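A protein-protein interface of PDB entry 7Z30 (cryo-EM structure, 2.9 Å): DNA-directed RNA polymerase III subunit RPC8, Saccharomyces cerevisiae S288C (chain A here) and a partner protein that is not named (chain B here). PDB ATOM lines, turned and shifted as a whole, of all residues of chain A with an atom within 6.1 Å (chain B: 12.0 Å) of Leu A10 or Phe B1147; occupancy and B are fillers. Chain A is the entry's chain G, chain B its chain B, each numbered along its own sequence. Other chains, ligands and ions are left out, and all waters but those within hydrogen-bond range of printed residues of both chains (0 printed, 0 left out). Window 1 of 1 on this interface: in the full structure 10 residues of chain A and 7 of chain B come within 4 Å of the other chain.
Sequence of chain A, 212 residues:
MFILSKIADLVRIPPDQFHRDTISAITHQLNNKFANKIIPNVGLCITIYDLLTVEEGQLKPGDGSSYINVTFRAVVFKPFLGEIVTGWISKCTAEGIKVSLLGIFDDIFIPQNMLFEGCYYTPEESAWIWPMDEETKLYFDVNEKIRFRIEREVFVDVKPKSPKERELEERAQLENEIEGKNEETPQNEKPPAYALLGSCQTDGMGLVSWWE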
ATOM      1  N   ALA A   8     -38.053 -11.637 -18.598  1.00  0.00           N
ATOM      2  CA  ALA A   8     -37.489 -12.944 -18.293  1.00  0.00           C
ATOM      3  C   ALA A   8     -36.159 -13.096 -19.015  1.00  0.00           C
ATOM      4  O   ALA A   8     -36.085 -12.917 -20.235  1.00  0.00           O
ATOM      5  CB  ALA A   8     -38.446 -14.064 -18.699  1.00  0.00           C
ATOM      6  N   ASP A   9     -35.112 -13.429 -18.265  1.00  0.00           N
ATOM      7  CA  ASP A   9     -33.782 -13.563 -18.840  1.00  0.00           C
ATOM      8  C   ASP A   9     -33.042 -14.705 -18.165  1.00  0.00           C
ATOM      9  O   ASP A   9     -33.372 -15.121 -17.051  1.00  0.00           O
ATOM     10  CB  ASP A   9     -32.980 -12.265 -18.711  1.00  0.00           C
ATOM     11  CG  ASP A   9     -31.929 -12.122 -19.793  1.00  0.00           C
ATOM     12  OD1 ASP A   9     -32.006 -12.851 -20.805  1.00  0.00           O
ATOM     13  OD2 ASP A   9     -31.024 -11.279 -19.634  1.00  0.00           O
ATOM     14  N   LEU A  10     -32.027 -15.205 -18.861  1.00  0.00           N
ATOM     15  CA  LEU A  10     -31.131 -16.230 -18.344  1.00  0.00           C
ATOM     16  C   LEU A  10     -29.880 -15.535 -17.830  1.00  0.00           C
ATOM     17  O   LEU A  10     -29.212 -14.819 -18.582  1.00  0.00           O
ATOM     18  CB  LEU A  10     -30.781 -17.250 -19.426  1.00  0.00           C
ATOM     19  CG  LEU A  10     -29.516 -18.073 -19.193  1.00  0.00           C
ATOM     20  CD1 LEU A  10     -29.838 -19.285 -18.343  1.00  0.00           C
ATOM     21  CD2 LEU A  10     -28.890 -18.485 -20.514  1.00  0.00           C
ATOM     22  N   VAL A  11     -29.569 -15.741 -16.560  1.00  0.00           N
ATOM     23  CA  VAL A  11     -28.500 -15.004 -15.902  1.00  0.00           C
ATOM     24  C   VAL A  11     -27.413 -15.975 -15.459  1.00  0.00           C
ATOM     25  O   VAL A  11     -27.685 -17.048 -14.907  1.00  0.00           O
ATOM     26  CB  VAL A  11     -29.056 -14.162 -14.730  1.00  0.00           C
ATOM     27  CG1 VAL A  11     -29.421 -15.023 -13.534  1.00  0.00           C
ATOM     28  CG2 VAL A  11     -28.076 -13.102 -14.342  1.00  0.00           C
ATOM     29  N   ARG A  12     -26.165 -15.612 -15.745  1.00  0.00           N
ATOM     30  CA  ARG A  12     -25.006 -16.456 -15.471  1.00  0.00           C
ATOM     31  C   ARG A  12     -24.261 -15.894 -14.268  1.00  0.00           C
ATOM     32  O   ARG A  12     -23.770 -14.762 -14.309  1.00  0.00           O
ATOM     33  CB  ARG A  12     -24.093 -16.544 -16.692  1.00  0.00           C
ATOM     34  CG  ARG A  12     -22.645 -16.876 -16.378  1.00  0.00           C
ATOM     35  CD  ARG A  12     -21.791 -16.818 -17.637  1.00  0.00           C
ATOM     36  NE  ARG A  12     -20.438 -17.326 -17.438  1.00  0.00           N
ATOM     37  CZ  ARG A  12     -19.525 -16.769 -16.653  1.00  0.00           C
ATOM     38  NH1 ARG A  12     -19.770 -15.653 -15.986  1.00  0.00           N
ATOM     39  NH2 ARG A  12     -18.329 -17.340 -16.544  1.00  0.00           N
ATOM     40  N   LYS A  33     -26.365  -6.134 -16.940  1.00  0.00           N
ATOM     41  CA  LYS A  33     -26.996  -6.283 -18.247  1.00  0.00           C
ATOM     42  C   LYS A  33     -28.011  -5.192 -18.575  1.00  0.00           C
ATOM     43  O   LYS A  33     -28.361  -5.032 -19.748  1.00  0.00           O
ATOM     44  CB  LYS A  33     -27.682  -7.647 -18.356  1.00  0.00           C
ATOM     45  CG  LYS A  33     -27.554  -8.279 -19.730  1.00  0.00           C
ATOM     46  CD  LYS A  33     -28.701  -9.225 -20.013  1.00  0.00           C
ATOM     47  CE  LYS A  33     -28.944  -9.372 -21.505  1.00  0.00           C
ATOM     48  NZ  LYS A  33     -27.700  -9.747 -22.226  1.00  0.00           N
ATOM     49  N   GLN A  58     -28.854 -24.052 -13.532  1.00  0.00           N
ATOM     50  CA  GLN A  58     -28.367 -25.229 -14.229  1.00  0.00           C
ATOM     51  C   GLN A  58     -26.998 -24.948 -14.833  1.00  0.00           C
ATOM     52  O   GLN A  58     -26.680 -23.812 -15.195  1.00  0.00           O
ATOM     53  CB  GLN A  58     -29.352 -25.669 -15.315  1.00  0.00           C
ATOM     54  CG  GLN A  58     -29.845 -24.544 -16.197  1.00  0.00           C
ATOM     55  CD  GLN A  58     -31.327 -24.645 -16.491  1.00  0.00           C
ATOM     56  OE1 GLN A  58     -31.819 -25.699 -16.893  1.00  0.00           O
ATOM     57  NE2 GLN A  58     -32.046 -23.549 -16.293  1.00  0.00           N
ATOM     58  N   LEU A  59     -26.189 -25.997 -14.932  1.00  0.00           N
ATOM     59  CA  LEU A  59     -24.799 -25.886 -15.349  1.00  0.00           C
ATOM     60  C   LEU A  59     -24.594 -26.619 -16.666  1.00  0.00           C
ATOM     61  O   LEU A  59     -25.062 -27.750 -16.831  1.00  0.00           O
ATOM     62  CB  LEU A  59     -23.864 -26.457 -14.281  1.00  0.00           C
ATOM     63  CG  LEU A  59     -23.753 -25.682 -12.967  1.00  0.00           C
ATOM     64  CD1 LEU A  59     -24.798 -26.146 -11.967  1.00  0.00           C
ATOM     65  CD2 LEU A  59     -22.361 -25.830 -12.390  1.00  0.00           C
ATOM     66  N   LYS A  60     -23.904 -25.972 -17.600  1.00  0.00           N
ATOM     67  CA  LYS A  60     -23.519 -26.646 -18.826  1.00  0.00           C
ATOM     68  C   LYS A  60     -22.230 -27.434 -18.595  1.00  0.00           C
ATOM     69  O   LYS A  60     -21.438 -27.097 -17.711  1.00  0.00           O
ATOM     70  CB  LYS A  60     -23.339 -25.642 -19.962  1.00  0.00           C
ATOM     71  CG  LYS A  60     -22.281 -24.595 -19.723  1.00  0.00           C
ATOM     72  CD  LYS A  60     -22.544 -23.363 -20.565  1.00  0.00           C
ATOM     73  CE  LYS A  60     -21.766 -23.400 -21.862  1.00  0.00           C
ATOM     74  NZ  LYS A  60     -22.035 -22.197 -22.691  1.00  0.00           N
ATOM     75  N   TYR A  67     -26.290 -20.903 -14.400  1.00  0.00           N
ATOM     76  CA  TYR A  67     -27.149 -20.201 -15.343  1.00  0.00           C
ATOM     77  C   TYR A  67     -28.582 -20.280 -14.836  1.00  0.00           C
ATOM     78  O   TYR A  67     -29.180 -21.360 -14.815  1.00  0.00           O
ATOM     79  CB  TYR A  67     -27.033 -20.798 -16.743  1.00  0.00           C
ATOM     80  CG  TYR A  67     -25.716 -20.518 -17.422  1.00  0.00           C
ATOM     81  CD1 TYR A  67     -24.595 -21.289 -17.152  1.00  0.00           C
ATOM     82  CD2 TYR A  67     -25.594 -19.485 -18.337  1.00  0.00           C
ATOM     83  CE1 TYR A  67     -23.391 -21.038 -17.774  1.00  0.00           C
ATOM     84  CE2 TYR A  67     -24.394 -19.226 -18.966  1.00  0.00           C
ATOM     85  CZ  TYR A  67     -23.297 -20.005 -18.681  1.00  0.00           C
ATOM     86  OH  TYR A  67     -22.100 -19.748 -19.306  1.00  0.00           O
ATOM     87  N   ILE A  68     -29.128 -19.136 -14.438  1.00  0.00           N
ATOM     88  CA  ILE A  68     -30.386 -19.068 -13.710  1.00  0.00           C
ATOM     89  C   ILE A  68     -31.423 -18.396 -14.596  1.00  0.00           C
ATOM     90  O   ILE A  68     -31.187 -17.296 -15.110  1.00  0.00           O
ATOM     91  CB  ILE A  68     -30.229 -18.306 -12.386  1.00  0.00           C
ATOM     92  CG1 ILE A  68     -29.084 -18.900 -11.565  1.00  0.00           C
ATOM     93  CG2 ILE A  68     -31.532 -18.309 -11.611  1.00  0.00           C
ATOM     94  CD1 ILE A  68     -28.973 -18.345 -10.175  1.00  0.00           C
ATOM     95  N   ASN A  69     -32.562 -19.056 -14.777  1.00  0.00           N
ATOM     96  CA  ASN A  69     -33.713 -18.423 -15.404  1.00  0.00           C
ATOM     97  C   ASN A  69     -34.454 -17.614 -14.349  1.00  0.00           C
ATOM     98  O   ASN A  69     -35.031 -18.183 -13.416  1.00  0.00           O
ATOM     99  CB  ASN A  69     -34.628 -19.472 -16.030  1.00  0.00           C
ATOM    100  CG  ASN A  69     -34.042 -20.076 -17.288  1.00  0.00           C
ATOM    101  OD1 ASN A  69     -33.076 -19.561 -17.847  1.00  0.00           O
ATOM    102  ND2 ASN A  69     -34.627 -21.177 -17.740  1.00  0.00           N
ATOM    103  N   VAL A  70     -34.438 -16.292 -14.493  1.00  0.00           N
ATOM    104  CA  VAL A  70     -34.975 -15.385 -13.489  1.00  0.00           C
ATOM    105  C   VAL A  70     -35.949 -14.426 -14.159  1.00  0.00           C
ATOM    106  O   VAL A  70     -35.727 -13.984 -15.291  1.00  0.00           O
ATOM    107  CB  VAL A  70     -33.848 -14.617 -12.762  1.00  0.00           C
ATOM    108  CG1 VAL A  70     -32.966 -13.884 -13.762  1.00  0.00           C
ATOM    109  CG2 VAL A  70     -34.420 -13.651 -11.729  1.00  0.00           C
ATOM    110  N   ASP B1096     -28.724 -18.172 -36.806  1.00  0.00           N
ATOM    111  CA  ASP B1096     -29.846 -18.962 -36.312  1.00  0.00           C
ATOM    112  C   ASP B1096     -30.921 -19.142 -37.374  1.00  0.00           C
ATOM    113  O   ASP B1096     -31.646 -20.142 -37.355  1.00  0.00           O
ATOM    114  CB  ASP B1096     -30.443 -18.314 -35.064  1.00  0.00           C
ATOM    115  CG  ASP B1096     -30.936 -19.334 -34.059  1.00  0.00           C
ATOM    116  OD1 ASP B1096     -31.116 -20.509 -34.440  1.00  0.00           O
ATOM    117  OD2 ASP B1096     -31.148 -18.962 -32.886  1.00  0.00           O
ATOM    118  N   ILE B1117     -24.976 -16.616 -33.998  1.00  0.00           N
ATOM    119  CA  ILE B1117     -24.692 -17.206 -32.699  1.00  0.00           C
ATOM    120  C   ILE B1117     -23.229 -17.650 -32.682  1.00  0.00           C
ATOM    121  O   ILE B1117     -22.655 -18.018 -33.705  1.00  0.00           O
ATOM    122  CB  ILE B1117     -25.639 -18.381 -32.381  1.00  0.00           C
ATOM    123  CG1 ILE B1117     -27.093 -17.920 -32.480  1.00  0.00           C
ATOM    124  CG2 ILE B1117     -25.381 -18.946 -30.992  1.00  0.00           C
ATOM    125  CD1 ILE B1117     -27.550 -17.089 -31.305  1.00  0.00           C
ATOM    126  N   LYS B1118     -22.629 -17.599 -31.493  1.00  0.00           N
ATOM    127  CA  LYS B1118     -21.225 -17.932 -31.293  1.00  0.00           C
ATOM    128  C   LYS B1118     -21.125 -19.271 -30.580  1.00  0.00           C
ATOM    129  O   LYS B1118     -21.716 -19.450 -29.509  1.00  0.00           O
ATOM    130  CB  LYS B1118     -20.517 -16.847 -30.472  1.00  0.00           C
ATOM    131  CG  LYS B1118     -19.044 -16.653 -30.798  1.00  0.00           C
ATOM    132  CD  LYS B1118     -18.851 -16.203 -32.233  1.00  0.00           C
ATOM    133  CE  LYS B1118     -17.600 -16.805 -32.853  1.00  0.00           C
ATOM    134  NZ  LYS B1118     -16.359 -16.113 -32.407  1.00  0.00           N
ATOM    135  N   MET B1119     -20.380 -20.205 -31.166  1.00  0.00           N
ATOM    136  CA  MET B1119     -20.159 -21.499 -30.538  1.00  0.00           C
ATOM    137  C   MET B1119     -18.841 -22.077 -31.030  1.00  0.00           C
ATOM    138  O   MET B1119     -18.297 -21.660 -32.055  1.00  0.00           O
ATOM    139  CB  MET B1119     -21.302 -22.473 -30.823  1.00  0.00           C
ATOM    140  CG  MET B1119     -21.860 -22.383 -32.223  1.00  0.00           C
ATOM    141  SD  MET B1119     -23.304 -23.436 -32.392  1.00  0.00           S
ATOM    142  CE  MET B1119     -22.686 -24.956 -31.677  1.00  0.00           C
ATOM    143  N   LEU B1143     -30.047 -24.895 -34.274  1.00  0.00           N
ATOM    144  CA  LEU B1143     -29.570 -24.693 -32.917  1.00  0.00           C
ATOM    145  C   LEU B1143     -30.731 -24.743 -31.936  1.00  0.00           C
ATOM    146  O   LEU B1143     -31.894 -24.578 -32.320  1.00  0.00           O
ATOM    147  CB  LEU B1143     -28.842 -23.360 -32.784  1.00  0.00           C
ATOM    148  CG  LEU B1143     -27.875 -23.028 -33.915  1.00  0.00           C
ATOM    149  CD1 LEU B1143     -27.766 -21.523 -34.067  1.00  0.00           C
ATOM    150  CD2 LEU B1143     -26.525 -23.660 -33.656  1.00  0.00           C
ATOM    151  N   GLU B1144     -30.402 -24.993 -30.675  1.00  0.00           N
ATOM    152  CA  GLU B1144     -31.336 -24.886 -29.570  1.00  0.00           C
ATOM    153  C   GLU B1144     -30.552 -24.528 -28.318  1.00  0.00           C
ATOM    154  O   GLU B1144     -29.357 -24.812 -28.211  1.00  0.00           O
ATOM    155  CB  GLU B1144     -32.120 -26.186 -29.345  1.00  0.00           C
ATOM    156  CG  GLU B1144     -31.249 -27.392 -29.042  1.00  0.00           C
ATOM    157  CD  GLU B1144     -32.027 -28.525 -28.403  1.00  0.00           C
ATOM    158  OE1 GLU B1144     -33.177 -28.291 -27.974  1.00  0.00           O
ATOM    159  OE2 GLU B1144     -31.488 -29.650 -28.328  1.00  0.00           O
ATOM    160  N   ASP B1145     -31.235 -23.904 -27.366  1.00  0.00           N
ATOM    161  CA  ASP B1145     -30.582 -23.539 -26.119  1.00  0.00           C
ATOM    162  C   ASP B1145     -30.321 -24.782 -25.280  1.00  0.00           C
ATOM    163  O   ASP B1145     -31.140 -25.703 -25.237  1.00  0.00           O
ATOM    164  CB  ASP B1145     -31.444 -22.554 -25.332  1.00  0.00           C
ATOM    165  CG  ASP B1145     -32.144 -21.552 -26.222  1.00  0.00           C
ATOM    166  OD1 ASP B1145     -33.033 -21.965 -26.996  1.00  0.00           O
ATOM    167  OD2 ASP B1145     -31.806 -20.353 -26.148  1.00  0.00           O
ATOM    168  N   ILE B1146     -29.166 -24.808 -24.613  1.00  0.00           N
ATOM    169  CA  ILE B1146     -28.938 -25.840 -23.607  1.00  0.00           C
ATOM    170  C   ILE B1146     -29.850 -25.609 -22.413  1.00  0.00           C
ATOM    171  O   ILE B1146     -30.302 -26.558 -21.760  1.00  0.00           O
ATOM    172  CB  ILE B1146     -27.457 -25.882 -23.185  1.00  0.00           C
ATOM    173  CG1 ILE B1146     -26.887 -24.477 -23.021  1.00  0.00           C
ATOM    174  CG2 ILE B1146     -26.625 -26.672 -24.171  1.00  0.00           C
ATOM    175  CD1 ILE B1146     -25.397 -24.482 -22.781  1.00  0.00           C
ATOM    176  N   PHE B1147     -30.136 -24.350 -22.114  1.00  0.00           N
ATOM    177  CA  PHE B1147     -30.914 -23.969 -20.953  1.00  0.00           C
ATOM    178  C   PHE B1147     -32.369 -23.751 -21.358  1.00  0.00           C
ATOM    179  O   PHE B1147     -32.786 -24.104 -22.466  1.00  0.00           O
ATOM    180  CB  PHE B1147     -30.272 -22.742 -20.309  1.00  0.00           C
ATOM    181  CG  PHE B1147     -28.818 -22.933 -20.003  1.00  0.00           C
ATOM    182  CD1 PHE B1147     -28.395 -24.028 -19.271  1.00  0.00           C
ATOM    183  CD2 PHE B1147     -27.871 -22.040 -20.470  1.00  0.00           C
ATOM    184  CE1 PHE B1147     -27.061 -24.222 -18.992  1.00  0.00           C
ATOM    185  CE2 PHE B1147     -26.532 -22.229 -20.196  1.00  0.00           C
ATOM    186  CZ  PHE B1147     -26.127 -23.323 -19.454  1.00  0.00           C
ATOM    187  N   GLN B1148     -33.157 -23.187 -20.442  1.00  0.00           N
ATOM    188  CA  GLN B1148     -34.612 -23.036 -20.494  1.00  0.00           C
ATOM    189  C   GLN B1148     -35.284 -24.391 -20.287  1.00  0.00           C
ATOM    190  O   GLN B1148     -36.517 -24.445 -20.169  1.00  0.00           O
ATOM    191  CB  GLN B1148     -35.117 -22.392 -21.797  1.00  0.00           C
ATOM    192  CG  GLN B1148     -36.541 -21.849 -21.749  1.00  0.00           C
ATOM    193  CD  GLN B1148     -36.843 -21.084 -20.474  1.00  0.00           C
ATOM    194  OE1 GLN B1148     -37.348 -21.647 -19.502  1.00  0.00           O
ATOM    195  NE2 GLN B1148     -36.537 -19.792 -20.474  1.00  0.00           N
ATOM    196  N   GLN B1149     -34.517 -25.478 -20.224  1.00  0.00           N
ATOM    197  CA  GLN B1149     -35.034 -26.810 -19.925  1.00  0.00           C
ATOM    198  C   GLN B1149     -36.095 -27.252 -20.929  1.00  0.00           C
ATOM    199  O   GLN B1149     -35.858 -27.246 -22.137  1.00  0.00           O
ATOM    200  CB  GLN B1149     -35.601 -26.847 -18.504  1.00  0.00           C
ATOM    201  CG  GLN B1149     -35.537 -28.207 -17.847  1.00  0.00           C
ATOM    202  CD  GLN B1149     -35.686 -28.123 -16.345  1.00  0.00           C
ATOM    203  OE1 GLN B1149     -36.154 -27.120 -15.809  1.00  0.00           O
ATOM    204  NE2 GLN B1149     -35.278 -29.179 -15.655  1.00  0.00           N
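CD2 of Phe B1147 touches CD2 of Leu A10, 3.7 Å away. Phe B1147 touches Gln A58. Ile B1146 touches Lys A60. CB of Lys A60 touches CZ of Phe B1147, 3.7 Å away. Phe B1147 touches Tyr A67 (CE2 to CG, 3.4 Å).
Of the 11 printed residues of chain B, 3 touch a printed residue of chain A. Printed residues of chain A that touch a printed residue of chain B: Leu A10, Gln A58, Lys A60, Tyr A67 and Asn A69. Among the printed residues, 6 pairs touch across the chains.
The side-chain amide oxygen (OE1) of Gln B1148 lies within hydrogen-bond range of the side-chain amide nitrogen (ND2) of Asn A69, at 3.3 Å.
O of Tyr A67 lies within hydrogen-bond range of N of Gln A58 (3.0 Å). OH of Tyr A67 lies close to NE of Arg A12, 3.5 Å away.
Of chain B, only Phe B1147 (3.7 Å) comes within 4 Å of Leu A10. Phe B1147 touches just these residues of chain A: Leu A10, Gln A58, Lys A60 and Tyr A67. No residue of chain B comes within 4 Å of Asp A9. No residue of chain B comes within 4 Å of Val A11. Gln A58 touches just one residue of chain B: Phe B1147 (3.4 Å). Lys A60 touches just these residues of chain B: Ile B1146 (3.7 Å) and Phe B1147 (3.7 Å). Of the printed residues of chain B, Tyr A67 touches Phe B1147. Of the printed residues of chain A, Ile B1146 touches Lys A60 (3.7 Å). Printed residues of chain A within 4 Å of Gln B1148: Asn A69. Ile A68 touches none of the printed residues of chain B. The nearest printed residue of chain A that does not touch Ile B1146 is Gln A58 (5.2 Å).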
